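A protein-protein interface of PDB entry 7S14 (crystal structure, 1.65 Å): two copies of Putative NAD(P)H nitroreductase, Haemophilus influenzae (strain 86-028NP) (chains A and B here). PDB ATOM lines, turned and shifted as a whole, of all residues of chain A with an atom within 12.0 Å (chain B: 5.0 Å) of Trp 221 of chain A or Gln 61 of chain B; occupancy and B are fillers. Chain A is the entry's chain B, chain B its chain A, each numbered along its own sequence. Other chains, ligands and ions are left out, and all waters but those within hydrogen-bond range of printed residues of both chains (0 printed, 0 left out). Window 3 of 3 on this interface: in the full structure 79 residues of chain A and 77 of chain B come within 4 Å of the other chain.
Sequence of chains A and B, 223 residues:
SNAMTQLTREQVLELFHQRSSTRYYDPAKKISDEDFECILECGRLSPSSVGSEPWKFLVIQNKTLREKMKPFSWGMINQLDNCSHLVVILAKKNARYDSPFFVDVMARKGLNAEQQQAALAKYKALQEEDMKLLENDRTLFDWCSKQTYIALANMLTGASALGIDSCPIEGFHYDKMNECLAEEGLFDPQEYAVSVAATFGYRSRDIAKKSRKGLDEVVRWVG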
ATOM      1  N   GLY A 214     -16.656  -3.032 -20.004  1.00  0.00           N
ATOM      2  CA  GLY A 214     -15.845  -3.765 -20.990  1.00  0.00           C
ATOM      3  C   GLY A 214     -16.623  -4.912 -21.604  1.00  0.00           C
ATOM      4  O   GLY A 214     -17.567  -5.418 -20.955  1.00  0.00           O
ATOM      5  N   LEU A 215     -16.237  -5.312 -22.815  1.00  0.00           N
ATOM      6  CA  LEU A 215     -16.811  -6.478 -23.534  1.00  0.00           C
ATOM      7  C   LEU A 215     -16.618  -7.737 -22.674  1.00  0.00           C
ATOM      8  O   LEU A 215     -17.533  -8.583 -22.666  1.00  0.00           O
ATOM      9  CB  LEU A 215     -16.135  -6.593 -24.906  1.00  0.00           C
ATOM     10  CG  LEU A 215     -16.996  -7.127 -26.051  1.00  0.00           C
ATOM     11  CD1 LEU A 215     -18.318  -6.382 -26.166  1.00  0.00           C
ATOM     12  CD2 LEU A 215     -16.239  -7.043 -27.367  1.00  0.00           C
ATOM     13  N   ASP A 216     -15.491  -7.829 -21.950  1.00  0.00           N
ATOM     14  CA  ASP A 216     -15.172  -8.924 -20.989  1.00  0.00           C
ATOM     15  C   ASP A 216     -16.285  -9.062 -19.941  1.00  0.00           C
ATOM     16  O   ASP A 216     -16.564 -10.207 -19.535  1.00  0.00           O
ATOM     17  CB  ASP A 216     -13.838  -8.683 -20.271  1.00  0.00           C
ATOM     18  CG  ASP A 216     -12.629  -9.316 -20.941  1.00  0.00           C
ATOM     19  OD1 ASP A 216     -12.780  -9.833 -22.064  1.00  0.00           O
ATOM     20  OD2 ASP A 216     -11.544  -9.295 -20.323  1.00  0.00           O
ATOM     21  N   GLU A 217     -16.870  -7.942 -19.505  1.00  0.00           N
ATOM     22  CA  GLU A 217     -17.849  -7.887 -18.384  1.00  0.00           C
ATOM     23  C   GLU A 217     -19.265  -8.197 -18.886  1.00  0.00           C
ATOM     24  O   GLU A 217     -20.018  -8.839 -18.130  1.00  0.00           O
ATOM     25  CB  GLU A 217     -17.816  -6.510 -17.719  1.00  0.00           C
ATOM     26  CG  GLU A 217     -18.643  -6.432 -16.447  1.00  0.00           C
ATOM     27  CD  GLU A 217     -18.410  -5.187 -15.608  1.00  0.00           C
ATOM     28  OE1 GLU A 217     -17.555  -4.359 -15.994  1.00  0.00           O
ATOM     29  OE2 GLU A 217     -19.085  -5.048 -14.568  1.00  0.00           O
ATOM     30  N   VAL A 218     -19.617  -7.751 -20.095  1.00  0.00           N
ATOM     31  CA  VAL A 218     -21.019  -7.790 -20.617  1.00  0.00           C
ATOM     32  C   VAL A 218     -21.247  -9.035 -21.485  1.00  0.00           C
ATOM     33  O   VAL A 218     -22.423  -9.411 -21.626  1.00  0.00           O
ATOM     34  CB  VAL A 218     -21.400  -6.501 -21.373  1.00  0.00           C
ATOM     35  CG1 VAL A 218     -21.273  -5.274 -20.484  1.00  0.00           C
ATOM     36  CG2 VAL A 218     -20.608  -6.319 -22.658  1.00  0.00           C
ATOM     37  N   VAL A 219     -20.200  -9.648 -22.053  1.00  0.00           N
ATOM     38  CA  VAL A 219     -20.350 -10.821 -22.969  1.00  0.00           C
ATOM     39  C   VAL A 219     -19.944 -12.099 -22.230  1.00  0.00           C
ATOM     40  O   VAL A 219     -18.791 -12.184 -21.772  1.00  0.00           O
ATOM     41  CB  VAL A 219     -19.546 -10.662 -24.276  1.00  0.00           C
ATOM     42  CG1 VAL A 219     -19.666 -11.891 -25.168  1.00  0.00           C
ATOM     43  CG2 VAL A 219     -19.964  -9.420 -25.044  1.00  0.00           C
ATOM     44  N   ARG A 220     -20.868 -13.058 -22.133  1.00  0.00           N
ATOM     45  CA  ARG A 220     -20.573 -14.464 -21.754  1.00  0.00           C
ATOM     46  C   ARG A 220     -20.650 -15.317 -23.023  1.00  0.00           C
ATOM     47  O   ARG A 220     -21.764 -15.449 -23.582  1.00  0.00           O
ATOM     48  CB  ARG A 220     -21.560 -14.940 -20.686  1.00  0.00           C
ATOM     49  CG  ARG A 220     -21.424 -16.405 -20.298  1.00  0.00           C
ATOM     50  CD  ARG A 220     -20.266 -16.691 -19.361  1.00  0.00           C
ATOM     51  NE  ARG A 220     -20.550 -17.912 -18.618  1.00  0.00           N
ATOM     52  CZ  ARG A 220     -20.451 -19.146 -19.106  1.00  0.00           C
ATOM     53  NH1 ARG A 220     -20.040 -19.357 -20.346  1.00  0.00           N
ATOM     54  NH2 ARG A 220     -20.763 -20.178 -18.342  1.00  0.00           N
ATOM     55  N   TRP A 221     -19.511 -15.849 -23.476  1.00  0.00           N
ATOM     56  CA  TRP A 221     -19.432 -16.725 -24.672  1.00  0.00           C
ATOM     57  C   TRP A 221     -19.768 -18.159 -24.250  1.00  0.00           C
ATOM     58  O   TRP A 221     -19.169 -18.645 -23.266  1.00  0.00           O
ATOM     59  CB  TRP A 221     -18.062 -16.633 -25.354  1.00  0.00           C
ATOM     60  CG  TRP A 221     -18.108 -17.049 -26.790  1.00  0.00           C
ATOM     61  CD1 TRP A 221     -18.122 -18.323 -27.278  1.00  0.00           C
ATOM     62  CD2 TRP A 221     -18.201 -16.182 -27.934  1.00  0.00           C
ATOM     63  NE1 TRP A 221     -18.196 -18.311 -28.645  1.00  0.00           N
ATOM     64  CE2 TRP A 221     -18.248 -17.010 -29.077  1.00  0.00           C
ATOM     65  CE3 TRP A 221     -18.239 -14.793 -28.106  1.00  0.00           C
ATOM     66  CZ2 TRP A 221     -18.327 -16.491 -30.368  1.00  0.00           C
ATOM     67  CZ3 TRP A 221     -18.315 -14.281 -29.382  1.00  0.00           C
ATOM     68  CH2 TRP A 221     -18.357 -15.120 -30.498  1.00  0.00           C
ATOM     69  N   VAL A 222     -20.716 -18.791 -24.947  1.00  0.00           N
ATOM     70  CA  VAL A 222     -21.175 -20.184 -24.667  1.00  0.00           C
ATOM     71  C   VAL A 222     -20.855 -21.044 -25.896  1.00  0.00           C
ATOM     72  O   VAL A 222     -21.771 -21.289 -26.719  1.00  0.00           O
ATOM     73  CB  VAL A 222     -22.671 -20.211 -24.294  1.00  0.00           C
ATOM     74  CG1 VAL A 222     -23.134 -21.606 -23.903  1.00  0.00           C
ATOM     75  CG2 VAL A 222     -22.986 -19.217 -23.184  1.00  0.00           C
ATOM     76  N   GLY A 223     -19.587 -21.449 -26.024  1.00  0.00           N
ATOM     77  CA  GLY A 223     -19.068 -22.231 -27.163  1.00  0.00           C
ATOM     78  C   GLY A 223     -19.271 -23.722 -26.957  1.00  0.00           C
ATOM     79  O   GLY A 223     -19.974 -24.367 -27.733  1.00  0.00           O
ATOM     80  N   PHE B  36     -18.270 -10.268 -35.917  1.00  0.00           N
ATOM     81  CA  PHE B  36     -19.210 -10.524 -34.797  1.00  0.00           C
ATOM     82  C   PHE B  36     -18.842  -9.673 -33.571  1.00  0.00           C
ATOM     83  O   PHE B  36     -19.764  -9.238 -32.863  1.00  0.00           O
ATOM     84  CB  PHE B  36     -19.345 -12.001 -34.428  1.00  0.00           C
ATOM     85  CG  PHE B  36     -20.522 -12.226 -33.514  1.00  0.00           C
ATOM     86  CD1 PHE B  36     -21.816 -12.036 -33.977  1.00  0.00           C
ATOM     87  CD2 PHE B  36     -20.338 -12.549 -32.179  1.00  0.00           C
ATOM     88  CE1 PHE B  36     -22.904 -12.201 -33.133  1.00  0.00           C
ATOM     89  CE2 PHE B  36     -21.428 -12.720 -31.339  1.00  0.00           C
ATOM     90  CZ  PHE B  36     -22.706 -12.549 -31.818  1.00  0.00           C
ATOM     91  N   GLU B  37     -17.549  -9.430 -33.332  1.00  0.00           N
ATOM     92  CA  GLU B  37     -17.074  -8.545 -32.231  1.00  0.00           C
ATOM     93  C   GLU B  37     -17.573  -7.115 -32.493  1.00  0.00           C
ATOM     94  O   GLU B  37     -17.972  -6.439 -31.523  1.00  0.00           O
ATOM     95  CB  GLU B  37     -15.551  -8.615 -32.086  1.00  0.00           C
ATOM     96  CG  GLU B  37     -15.045  -9.955 -31.571  1.00  0.00           C
ATOM     97  CD  GLU B  37     -15.038 -10.121 -30.059  1.00  0.00           C
ATOM     98  OE1 GLU B  37     -14.241  -9.431 -29.397  1.00  0.00           O
ATOM     99  OE2 GLU B  37     -15.828 -10.940 -29.547  1.00  0.00           O
ATOM    100  N   LEU B  40     -21.166  -6.981 -31.441  1.00  0.00           N
ATOM    101  CA  LEU B  40     -21.248  -6.946 -29.956  1.00  0.00           C
ATOM    102  C   LEU B  40     -20.909  -5.537 -29.461  1.00  0.00           C
ATOM    103  O   LEU B  40     -21.634  -5.042 -28.576  1.00  0.00           O
ATOM    104  CB  LEU B  40     -20.335  -8.018 -29.358  1.00  0.00           C
ATOM    105  CG  LEU B  40     -20.839  -9.445 -29.559  1.00  0.00           C
ATOM    106  CD1 LEU B  40     -19.784 -10.454 -29.142  1.00  0.00           C
ATOM    107  CD2 LEU B  40     -22.137  -9.673 -28.796  1.00  0.00           C
ATOM    108  N   VAL B  59     -23.698 -15.330 -25.870  1.00  0.00           N
ATOM    109  CA  VAL B  59     -23.507 -15.778 -27.282  1.00  0.00           C
ATOM    110  C   VAL B  59     -23.565 -17.307 -27.283  1.00  0.00           C
ATOM    111  O   VAL B  59     -22.571 -17.938 -26.887  1.00  0.00           O
ATOM    112  CB  VAL B  59     -22.204 -15.230 -27.892  1.00  0.00           C
ATOM    113  CG1 VAL B  59     -22.106 -15.545 -29.377  1.00  0.00           C
ATOM    114  CG2 VAL B  59     -22.066 -13.733 -27.656  1.00  0.00           C
ATOM    115  N   ILE B  60     -24.709 -17.873 -27.679  1.00  0.00           N
ATOM    116  CA  ILE B  60     -24.982 -19.337 -27.577  1.00  0.00           C
ATOM    117  C   ILE B  60     -24.574 -19.996 -28.899  1.00  0.00           C
ATOM    118  O   ILE B  60     -25.418 -20.056 -29.818  1.00  0.00           O
ATOM    119  CB  ILE B  60     -26.455 -19.608 -27.213  1.00  0.00           C
ATOM    120  CG1 ILE B  60     -26.912 -18.802 -25.992  1.00  0.00           C
ATOM    121  CG2 ILE B  60     -26.695 -21.097 -27.030  1.00  0.00           C
ATOM    122  CD1 ILE B  60     -26.384 -19.304 -24.672  1.00  0.00           C
ATOM    123  N   GLN B  61     -23.323 -20.459 -28.985  1.00  0.00           N
ATOM    124  CA  GLN B  61     -22.768 -21.131 -30.191  1.00  0.00           C
ATOM    125  C   GLN B  61     -22.858 -22.650 -30.027  1.00  0.00           C
ATOM    126  O   GLN B  61     -22.756 -23.353 -31.049  1.00  0.00           O
ATOM    127  CB  GLN B  61     -21.325 -20.683 -30.429  1.00  0.00           C
ATOM    128  CG  GLN B  61     -21.192 -19.206 -30.772  1.00  0.00           C
ATOM    129  CD  GLN B  61     -22.154 -18.779 -31.856  1.00  0.00           C
ATOM    130  OE1 GLN B  61     -23.295 -18.412 -31.586  1.00  0.00           O
ATOM    131  NE2 GLN B  61     -21.701 -18.834 -33.099  1.00  0.00           N
ATOM    132  N   ASN B  62     -23.047 -23.126 -28.793  1.00  0.00           N
ATOM    133  CA  ASN B  62     -23.103 -24.571 -28.454  1.00  0.00           C
ATOM    134  C   ASN B  62     -24.318 -25.206 -29.137  1.00  0.00           C
ATOM    135  O   ASN B  62     -25.447 -24.813 -28.807  1.00  0.00           O
ATOM    136  CB  ASN B  62     -23.142 -24.788 -26.941  1.00  0.00           C
ATOM    137  CG  ASN B  62     -23.009 -26.249 -26.580  1.00  0.00           C
ATOM    138  OD1 ASN B  62     -23.989 -26.990 -26.615  1.00  0.00           O
ATOM    139  ND2 ASN B  62     -21.797 -26.675 -26.258  1.00  0.00           N
ATOM    140  N   LYS B  63     -24.081 -26.166 -30.037  1.00  0.00           N
ATOM    141  CA  LYS B  63     -25.129 -26.791 -30.891  1.00  0.00           C
ATOM    142  C   LYS B  63     -26.042 -27.675 -30.036  1.00  0.00           C
ATOM    143  O   LYS B  63     -27.224 -27.802 -30.391  1.00  0.00           O
ATOM    144  CB  LYS B  63     -24.490 -27.584 -32.035  1.00  0.00           C
ATOM    145  CG  LYS B  63     -23.911 -26.726 -33.153  1.00  0.00           C
ATOM    146  CD  LYS B  63     -23.166 -27.520 -34.202  1.00  0.00           C
ATOM    147  CE  LYS B  63     -22.588 -26.645 -35.296  1.00  0.00           C
ATOM    148  NZ  LYS B  63     -23.556 -26.434 -36.396  1.00  0.00           N
ATOM    149  N   ARG B  66     -28.380 -25.244 -28.287  1.00  0.00           N
ATOM    150  CA  ARG B  66     -29.296 -24.765 -29.360  1.00  0.00           C
ATOM    151  C   ARG B  66     -30.415 -25.787 -29.574  1.00  0.00           C
ATOM    152  O   ARG B  66     -31.574 -25.358 -29.699  1.00  0.00           O
ATOM    153  CB  ARG B  66     -28.536 -24.499 -30.661  1.00  0.00           C
ATOM    154  CG  ARG B  66     -27.744 -23.201 -30.649  1.00  0.00           C
ATOM    155  CD  ARG B  66     -27.350 -22.802 -32.052  1.00  0.00           C
ATOM    156  NE  ARG B  66     -26.496 -21.626 -32.080  1.00  0.00           N
ATOM    157  CZ  ARG B  66     -26.000 -21.080 -33.186  1.00  0.00           C
ATOM    158  NH1 ARG B  66     -26.272 -21.603 -34.372  1.00  0.00           N
ATOM    159  NH2 ARG B  66     -25.230 -20.011 -33.101  1.00  0.00           N
ATOM    160  N   SER B  84     -25.718 -18.419 -37.893  1.00  0.00           N
ATOM    161  CA  SER B  84     -24.275 -18.337 -37.547  1.00  0.00           C
ATOM    162  C   SER B  84     -24.132 -18.128 -36.039  1.00  0.00           C
ATOM    163  O   SER B  84     -23.569 -19.008 -35.362  1.00  0.00           O
ATOM    164  CB  SER B  84     -23.584 -17.241 -38.311  1.00  0.00           C
ATOM    165  OG  SER B  84     -22.219 -17.160 -37.932  1.00  0.00           O
ATOM    166  N   HIS B  85     -24.673 -17.019 -35.540  1.00  0.00           N
ATOM    167  CA  HIS B  85     -24.583 -16.608 -34.116  1.00  0.00           C
ATOM    168  C   HIS B  85     -25.985 -16.404 -33.546  1.00  0.00           C
ATOM    169  O   HIS B  85     -26.880 -15.937 -34.282  1.00  0.00           O
ATOM    170  CB  HIS B  85     -23.723 -15.347 -33.974  1.00  0.00           C
ATOM    171  CG  HIS B  85     -22.274 -15.591 -34.221  1.00  0.00           C
ATOM    172  ND1 HIS B  85     -21.796 -15.966 -35.458  1.00  0.00           N
ATOM    173  CD2 HIS B  85     -21.202 -15.521 -33.402  1.00  0.00           C
ATOM    174  CE1 HIS B  85     -20.487 -16.117 -35.395  1.00  0.00           C
ATOM    175  NE2 HIS B  85     -20.097 -15.856 -34.139  1.00  0.00           N
ATOM    176  N   LEU B  86     -26.140 -16.746 -32.270  1.00  0.00           N
ATOM    177  CA  LEU B  86     -27.354 -16.496 -31.459  1.00  0.00           C
ATOM    178  C   LEU B  86     -26.919 -15.715 -30.218  1.00  0.00           C
ATOM    179  O   LEU B  86     -25.924 -16.116 -29.586  1.00  0.00           O
ATOM    180  CB  LEU B  86     -27.987 -17.842 -31.098  1.00  0.00           C
ATOM    181  CG  LEU B  86     -29.075 -17.811 -30.024  1.00  0.00           C
ATOM    182  CD1 LEU B  86     -30.252 -16.949 -30.451  1.00  0.00           C
ATOM    183  CD2 LEU B  86     -29.540 -19.219 -29.704  1.00  0.00           C
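The backbone NH (N) of Val 59 of chain B lies within hydrogen-bond range of the backbone carbonyl oxygen (O) of Arg 220 of chain A (3.0 Å).
The side-chain amide nitrogen (ND2) of Asn 62 of chain B sits close to the backbone carbonyl oxygen (O) of Gly 223 of chain A, 3.3 Å away.
O of Val 59 of chain B is in hydrogen-bond range of N of Val 222 of chain A (2.8 Å).
The backbone NH of Asn 62 of chain B is in hydrogen-bond range of the backbone carbonyl oxygen of Val 222 of chain A, 3.1 Å away.
N of Gln 61 of chain B is in hydrogen-bond range of O of Val 222 of chain A (2.9 Å).
O of Ile 60 of chain B is in hydrogen-bond range of NE of Arg 66 of chain B (3.0 Å).
The backbone NH (N) of Leu 86 of chain B lies within hydrogen-bond range of the side-chain amide oxygen (OE1) of Gln 61 of chain B, 3.4 Å away.
The backbone carbonyl oxygen (O) of Ser 84 of chain B lies within hydrogen-bond range of the side-chain amide nitrogen (NE2) of Gln 61 of chain B.
The side-chain amide oxygen (OE1) of Gln 61 of chain B sits at hydrogen-bond distance from the guanidinium group (NH2) of Arg 66 of chain B, 2.9 Å away.
N of Ile 60 of chain B sits at hydrogen-bond distance from O of Leu 86 of chain B, at 2.9 Å.
Of the 12 printed residues of chain B, 6 touch a printed residue of chain A.
Hydrophobic or aromatic side chains of chain B that line the printed part of chain A: Phe 36, Val 59 and Ile 60.
Of the 10 printed residues of chain A, 6 touch a printed residue of chain B.
Printed residues of chain A that touch a printed residue of chain B: Leu 215, Val 219, Arg 220, Trp 221, Val 222 and Gly 223.
Hydrophobic or aromatic side chains of chain A within 4 Å of the printed part of chain B: Leu 215, Val 219, Trp 221 and Val 222.
Among the printed residues, no Asp or Glu carboxylate lies within 4 Å of a Lys or Arg side-chain nitrogen of the other chain.
Among the printed residues, pairs that only touch across the chains: Trp 221 of chain A with Phe 36 of chain B, Val 222 of chain A with Ile 60 of chain B, Leu 215 of chain A with Glu 37 of chain B, Trp 221 of chain A with Gln 61 of chain B, Trp 221 of chain A with Val 59 of chain B and Val 219 of chain A with Val 59 of chain B.
No position is printed for both chains.
Of the 11 pairs that touch across the chains among the printed residues, none has its exchanged pair printed and touching as well.
Gly 214 of chain A touches none of the printed residues of chain B.
Of the printed residues of chain B, Leu 215 of chain A touches Glu 37 (3.7 Å).
Val 218 of chain A touches none of the printed residues of chain B.
Printed residues of chain B within 4 Å of Val 219 of chain A: Val 59 (3.9 Å).
Trp 221 of chain A touches three residues of chain B.
Printed residues of chain B within 4 Å of Val 222 of chain A: Val 59 (2.8 Å), Ile 60 (3.7 Å), Gln 61 (2.9 Å) and Asn 62 (3.1 Å).
Printed residues of chain B within 4 Å of Gly 223 of chain A: Asn 62 (3.2 Å).
Phe 36 of chain B touches one residue of chain A.
Of the printed residues of chain A, Glu 37 of chain B touches Leu 215.
Printed residues of chain A within 4 Å of Val 59 of chain B: Val 219 (3.9 Å), Arg 220 (3.0 Å), Trp 221 (3.9 Å) and Val 222 (2.8 Å).
Ile 60 of chain B touches just one residue of chain A: Val 222.
Gln 61 of chain B touches just these residues of chain A: Trp 221 and Val 222.
Of chain A, only Val 222 and Gly 223 come within 4 Å of Asn 62 of chain B.
No residue of chain A comes within 4 Å of Lys 63 of chain B.
No residue of chain A comes within 4 Å of Ser 84 of chain B.
No residue of chain A comes within 4 Å of His 85 of chain B.
No residue of chain A comes within 4 Å of Leu 86 of chain B.
The nearest printed residue of chain A that does not touch Glu 37 of chain B is Trp 221 of chain A (4.2 Å).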
